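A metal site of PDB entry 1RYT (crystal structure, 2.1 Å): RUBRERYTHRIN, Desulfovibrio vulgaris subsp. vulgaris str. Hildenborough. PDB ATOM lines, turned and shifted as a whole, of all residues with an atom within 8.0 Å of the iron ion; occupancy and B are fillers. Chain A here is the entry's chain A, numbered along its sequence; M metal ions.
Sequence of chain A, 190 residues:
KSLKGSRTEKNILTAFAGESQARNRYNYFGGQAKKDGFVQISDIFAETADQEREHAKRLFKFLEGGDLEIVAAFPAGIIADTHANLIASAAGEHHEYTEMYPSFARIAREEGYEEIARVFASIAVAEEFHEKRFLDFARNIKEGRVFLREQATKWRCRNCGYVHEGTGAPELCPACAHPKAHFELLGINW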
ATOM      1  N   ARG A 156     -33.138  21.618  11.175  1.00  0.00           N
ATOM      2  CA  ARG A 156     -32.640  21.835  12.527  1.00  0.00           C
ATOM      3  C   ARG A 156     -31.148  21.518  12.689  1.00  0.00           C
ATOM      4  O   ARG A 156     -30.656  20.498  12.204  1.00  0.00           O
ATOM      5  CB  ARG A 156     -33.449  21.042  13.538  1.00  0.00           C
ATOM      6  CG  ARG A 156     -33.202  21.453  14.980  1.00  0.00           C
ATOM      7  CD  ARG A 156     -33.805  20.471  15.968  1.00  0.00           C
ATOM      8  NE  ARG A 156     -33.135  19.179  15.909  1.00  0.00           N
ATOM      9  CZ  ARG A 156     -32.619  18.538  16.952  1.00  0.00           C
ATOM     10  NH1 ARG A 156     -32.702  19.046  18.166  1.00  0.00           N
ATOM     11  NH2 ARG A 156     -32.032  17.367  16.775  1.00  0.00           N
ATOM     12  N   CYS A 157     -30.432  22.448  13.320  1.00  0.00           N
ATOM     13  CA  CYS A 157     -29.009  22.282  13.633  1.00  0.00           C
ATOM     14  C   CYS A 157     -28.976  21.375  14.854  1.00  0.00           C
ATOM     15  O   CYS A 157     -29.497  21.713  15.917  1.00  0.00           O
ATOM     16  CB  CYS A 157     -28.391  23.647  13.972  1.00  0.00           C
ATOM     17  SG  CYS A 157     -26.644  23.627  14.542  1.00  0.00           S
ATOM     18  N   ARG A 158     -28.387  20.198  14.689  1.00  0.00           N
ATOM     19  CA  ARG A 158     -28.299  19.237  15.782  1.00  0.00           C
ATOM     20  C   ARG A 158     -27.355  19.724  16.887  1.00  0.00           C
ATOM     21  O   ARG A 158     -27.475  19.308  18.032  1.00  0.00           O
ATOM     22  CB  ARG A 158     -27.831  17.888  15.275  1.00  0.00           C
ATOM     23  CG  ARG A 158     -28.591  17.362  14.107  1.00  0.00           C
ATOM     24  CD  ARG A 158     -28.021  16.057  13.639  1.00  0.00           C
ATOM     25  NE  ARG A 158     -28.518  14.918  14.403  1.00  0.00           N
ATOM     26  CZ  ARG A 158     -27.839  14.325  15.379  1.00  0.00           C
ATOM     27  NH1 ARG A 158     -26.646  14.769  15.739  1.00  0.00           N
ATOM     28  NH2 ARG A 158     -28.379  13.284  16.015  1.00  0.00           N
ATOM     29  N   ASN A 159     -26.467  20.657  16.557  1.00  0.00           N
ATOM     30  CA  ASN A 159     -25.528  21.182  17.554  1.00  0.00           C
ATOM     31  C   ASN A 159     -26.157  22.197  18.520  1.00  0.00           C
ATOM     32  O   ASN A 159     -25.937  22.121  19.730  1.00  0.00           O
ATOM     33  CB  ASN A 159     -24.323  21.804  16.835  1.00  0.00           C
ATOM     34  CG  ASN A 159     -23.173  22.113  17.797  1.00  0.00           C
ATOM     35  OD1 ASN A 159     -22.706  23.241  17.874  1.00  0.00           O
ATOM     36  ND2 ASN A 159     -22.713  21.089  18.495  1.00  0.00           N
ATOM     37  N   CYS A 160     -26.939  23.130  18.020  1.00  0.00           N
ATOM     38  CA  CYS A 160     -27.518  24.125  18.928  1.00  0.00           C
ATOM     39  C   CYS A 160     -29.040  24.176  18.892  1.00  0.00           C
ATOM     40  O   CYS A 160     -29.630  24.875  19.711  1.00  0.00           O
ATOM     41  CB  CYS A 160     -26.951  25.511  18.635  1.00  0.00           C
ATOM     42  SG  CYS A 160     -27.489  26.224  17.055  1.00  0.00           S
ATOM     43  N   GLY A 161     -29.674  23.458  17.960  1.00  0.00           N
ATOM     44  CA  GLY A 161     -31.131  23.447  17.867  1.00  0.00           C
ATOM     45  C   GLY A 161     -31.803  24.573  17.092  1.00  0.00           C
ATOM     46  O   GLY A 161     -33.031  24.705  17.109  1.00  0.00           O
ATOM     47  N   TYR A 162     -31.007  25.376  16.387  1.00  0.00           N
ATOM     48  CA  TYR A 162     -31.526  26.490  15.598  1.00  0.00           C
ATOM     49  C   TYR A 162     -32.411  25.929  14.480  1.00  0.00           C
ATOM     50  O   TYR A 162     -31.980  25.007  13.768  1.00  0.00           O
ATOM     51  CB  TYR A 162     -30.365  27.312  15.007  1.00  0.00           C
ATOM     52  CG  TYR A 162     -30.791  28.408  14.028  1.00  0.00           C
ATOM     53  CD1 TYR A 162     -31.254  29.647  14.485  1.00  0.00           C
ATOM     54  CD2 TYR A 162     -30.753  28.186  12.642  1.00  0.00           C
ATOM     55  CE1 TYR A 162     -31.655  30.641  13.589  1.00  0.00           C
ATOM     56  CE2 TYR A 162     -31.176  29.178  11.742  1.00  0.00           C
ATOM     57  CZ  TYR A 162     -31.615  30.385  12.227  1.00  0.00           C
ATOM     58  OH  TYR A 162     -32.000  31.376  11.342  1.00  0.00           O
ATOM     59  N   VAL A 163     -33.634  26.438  14.364  1.00  0.00           N
ATOM     60  CA  VAL A 163     -34.568  25.997  13.308  1.00  0.00           C
ATOM     61  C   VAL A 163     -34.510  26.977  12.132  1.00  0.00           C
ATOM     62  O   VAL A 163     -34.553  28.194  12.313  1.00  0.00           O
ATOM     63  CB  VAL A 163     -36.021  25.824  13.795  1.00  0.00           C
ATOM     64  CG1 VAL A 163     -36.940  25.460  12.629  1.00  0.00           C
ATOM     65  CG2 VAL A 163     -36.062  24.736  14.851  1.00  0.00           C
ATOM     66  N   LEU A 172     -23.602  27.910   7.231  1.00  0.00           N
ATOM     67  CA  LEU A 172     -23.139  27.931   8.606  1.00  0.00           C
ATOM     68  C   LEU A 172     -24.360  28.269   9.443  1.00  0.00           C
ATOM     69  O   LEU A 172     -25.167  29.095   9.043  1.00  0.00           O
ATOM     70  CB  LEU A 172     -22.120  29.044   8.840  1.00  0.00           C
ATOM     71  CG  LEU A 172     -20.705  28.928   8.288  1.00  0.00           C
ATOM     72  CD1 LEU A 172     -20.031  30.271   8.433  1.00  0.00           C
ATOM     73  CD2 LEU A 172     -19.919  27.867   9.037  1.00  0.00           C
ATOM     74  N   CYS A 173     -24.503  27.625  10.588  1.00  0.00           N
ATOM     75  CA  CYS A 173     -25.620  27.928  11.444  1.00  0.00           C
ATOM     76  C   CYS A 173     -25.419  29.325  12.039  1.00  0.00           C
ATOM     77  O   CYS A 173     -24.336  29.620  12.560  1.00  0.00           O
ATOM     78  CB  CYS A 173     -25.705  26.905  12.560  1.00  0.00           C
ATOM     79  SG  CYS A 173     -26.805  27.385  13.874  1.00  0.00           S
ATOM     80  N   PRO A 174     -26.430  30.217  11.969  1.00  0.00           N
ATOM     81  CA  PRO A 174     -26.243  31.568  12.539  1.00  0.00           C
ATOM     82  C   PRO A 174     -26.141  31.717  14.059  1.00  0.00           C
ATOM     83  O   PRO A 174     -25.673  32.746  14.557  1.00  0.00           O
ATOM     84  CB  PRO A 174     -27.430  32.353  11.970  1.00  0.00           C
ATOM     85  CG  PRO A 174     -28.463  31.317  11.687  1.00  0.00           C
ATOM     86  CD  PRO A 174     -27.682  30.130  11.188  1.00  0.00           C
ATOM     87  N   ALA A 175     -26.588  30.700  14.796  1.00  0.00           N
ATOM     88  CA  ALA A 175     -26.538  30.722  16.257  1.00  0.00           C
ATOM     89  C   ALA A 175     -25.194  30.197  16.782  1.00  0.00           C
ATOM     90  O   ALA A 175     -24.461  30.921  17.429  1.00  0.00           O
ATOM     91  CB  ALA A 175     -27.706  29.921  16.827  1.00  0.00           C
ATOM     92  N   CYS A 176     -24.854  28.947  16.447  1.00  0.00           N
ATOM     93  CA  CYS A 176     -23.605  28.324  16.909  1.00  0.00           C
ATOM     94  C   CYS A 176     -22.452  28.390  15.925  1.00  0.00           C
ATOM     95  O   CYS A 176     -21.375  27.874  16.218  1.00  0.00           O
ATOM     96  CB  CYS A 176     -23.839  26.865  17.307  1.00  0.00           C
ATOM     97  SG  CYS A 176     -24.010  25.758  15.897  1.00  0.00           S
ATOM     98  N   ALA A 177     -22.685  28.936  14.735  1.00  0.00           N
ATOM     99  CA  ALA A 177     -21.632  29.051  13.731  1.00  0.00           C
ATOM    100  C   ALA A 177     -20.979  27.749  13.286  1.00  0.00           C
ATOM    101  O   ALA A 177     -19.822  27.737  12.849  1.00  0.00           O
ATOM    102  CB  ALA A 177     -20.586  30.044  14.181  1.00  0.00           C
ATOM    103  N   HIS A 178     -21.682  26.629  13.464  1.00  0.00           N
ATOM    104  CA  HIS A 178     -21.164  25.347  13.024  1.00  0.00           C
ATOM    105  C   HIS A 178     -21.663  25.198  11.600  1.00  0.00           C
ATOM    106  O   HIS A 178     -22.672  25.797  11.228  1.00  0.00           O
ATOM    107  CB  HIS A 178     -21.615  24.218  13.972  1.00  0.00           C
ATOM    108  CG  HIS A 178     -20.768  24.113  15.206  1.00  0.00           C
ATOM    109  ND1 HIS A 178     -20.454  25.193  15.993  1.00  0.00           N
ATOM    110  CD2 HIS A 178     -20.141  23.051  15.760  1.00  0.00           C
ATOM    111  CE1 HIS A 178     -19.666  24.802  16.981  1.00  0.00           C
ATOM    112  NE2 HIS A 178     -19.459  23.505  16.864  1.00  0.00           N
ATOM    113  N   PRO A 179     -20.933  24.471  10.747  1.00  0.00           N
ATOM    114  CA  PRO A 179     -21.383  24.314   9.356  1.00  0.00           C
ATOM    115  C   PRO A 179     -22.608  23.461   9.020  1.00  0.00           C
ATOM    116  O   PRO A 179     -23.158  22.733   9.866  1.00  0.00           O
ATOM    117  CB  PRO A 179     -20.123  23.769   8.664  1.00  0.00           C
ATOM    118  CG  PRO A 179     -19.475  22.974   9.747  1.00  0.00           C
ATOM    119  CD  PRO A 179     -19.618  23.855  10.955  1.00  0.00           C
ATOM    120  N   HIS A 182     -24.051  19.957  10.118  1.00  0.00           N
ATOM    121  CA  HIS A 182     -24.807  19.735  11.361  1.00  0.00           C
ATOM    122  C   HIS A 182     -26.310  19.793  11.316  1.00  0.00           C
ATOM    123  O   HIS A 182     -26.967  19.506  12.329  1.00  0.00           O
ATOM    124  CB  HIS A 182     -24.313  20.703  12.446  1.00  0.00           C
ATOM    125  CG  HIS A 182     -22.953  20.385  12.941  1.00  0.00           C
ATOM    126  ND1 HIS A 182     -22.728  19.507  13.979  1.00  0.00           N
ATOM    127  CD2 HIS A 182     -21.722  20.766  12.504  1.00  0.00           C
ATOM    128  CE1 HIS A 182     -21.430  19.351  14.156  1.00  0.00           C
ATOM    129  NE2 HIS A 182     -20.803  20.108  13.276  1.00  0.00           N
ATOM    130  N   PHE A 183     -26.851  20.170  10.162  1.00  0.00           N
ATOM    131  CA  PHE A 183     -28.288  20.308   9.949  1.00  0.00           C
ATOM    132  C   PHE A 183     -29.013  19.024   9.519  1.00  0.00           C
ATOM    133  O   PHE A 183     -28.466  18.174   8.814  1.00  0.00           O
ATOM    134  CB  PHE A 183     -28.528  21.426   8.918  1.00  0.00           C
ATOM    135  CG  PHE A 183     -28.498  22.808   9.510  1.00  0.00           C
ATOM    136  CD1 PHE A 183     -27.307  23.511   9.630  1.00  0.00           C
ATOM    137  CD2 PHE A 183     -29.670  23.406   9.980  1.00  0.00           C
ATOM    138  CE1 PHE A 183     -27.291  24.790  10.220  1.00  0.00           C
ATOM    139  CE2 PHE A 183     -29.659  24.672  10.572  1.00  0.00           C
ATOM    140  CZ  PHE A 183     -28.466  25.366  10.688  1.00  0.00           C
HETATM  141 FE    FE M   1     -26.353  25.631  15.377  1.00  0.00          FE
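Of the 18 residues printed, 4 come within 4 Å of the iron ion. The nearest printed residue that does not touch the iron ion is Tyr 162 (4.4 Å).
SG of Cys 160 is bound to the iron ion (2.1 Å). SG of Cys 157 is bound to the iron ion (2.2 Å). The iron ion is bound by the side-chain sulfur (SG) of Cys 173 (2.4 Å). SG of Cys 176 is bound to the iron ion (2.4 Å).
SG of Cys 160 sits close to N of Tyr 162. The backbone carbonyl oxygen of Tyr 162 lies within hydrogen-bond range of the backbone NH of Cys 157, at 3.0 Å. SG of Cys 157 sits close to N of Asn 159, at 3.6 Å. The side-chain sulfur of Cys 173 sits close to the backbone NH of Ala 175, 3.4 Å away. The backbone carbonyl oxygen (O) of His 178 lies within hydrogen-bond range of the backbone NH (N) of Cys 173 (2.7 Å). The side-chain sulfur (SG) of Cys 176 sits close to the side-chain amide oxygen (OD1) of Asn 159 (3.5 Å). The backbone carbonyl oxygen (O) of Cys 176 lies within hydrogen-bond range of a ring nitrogen (ND1) of His 178.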
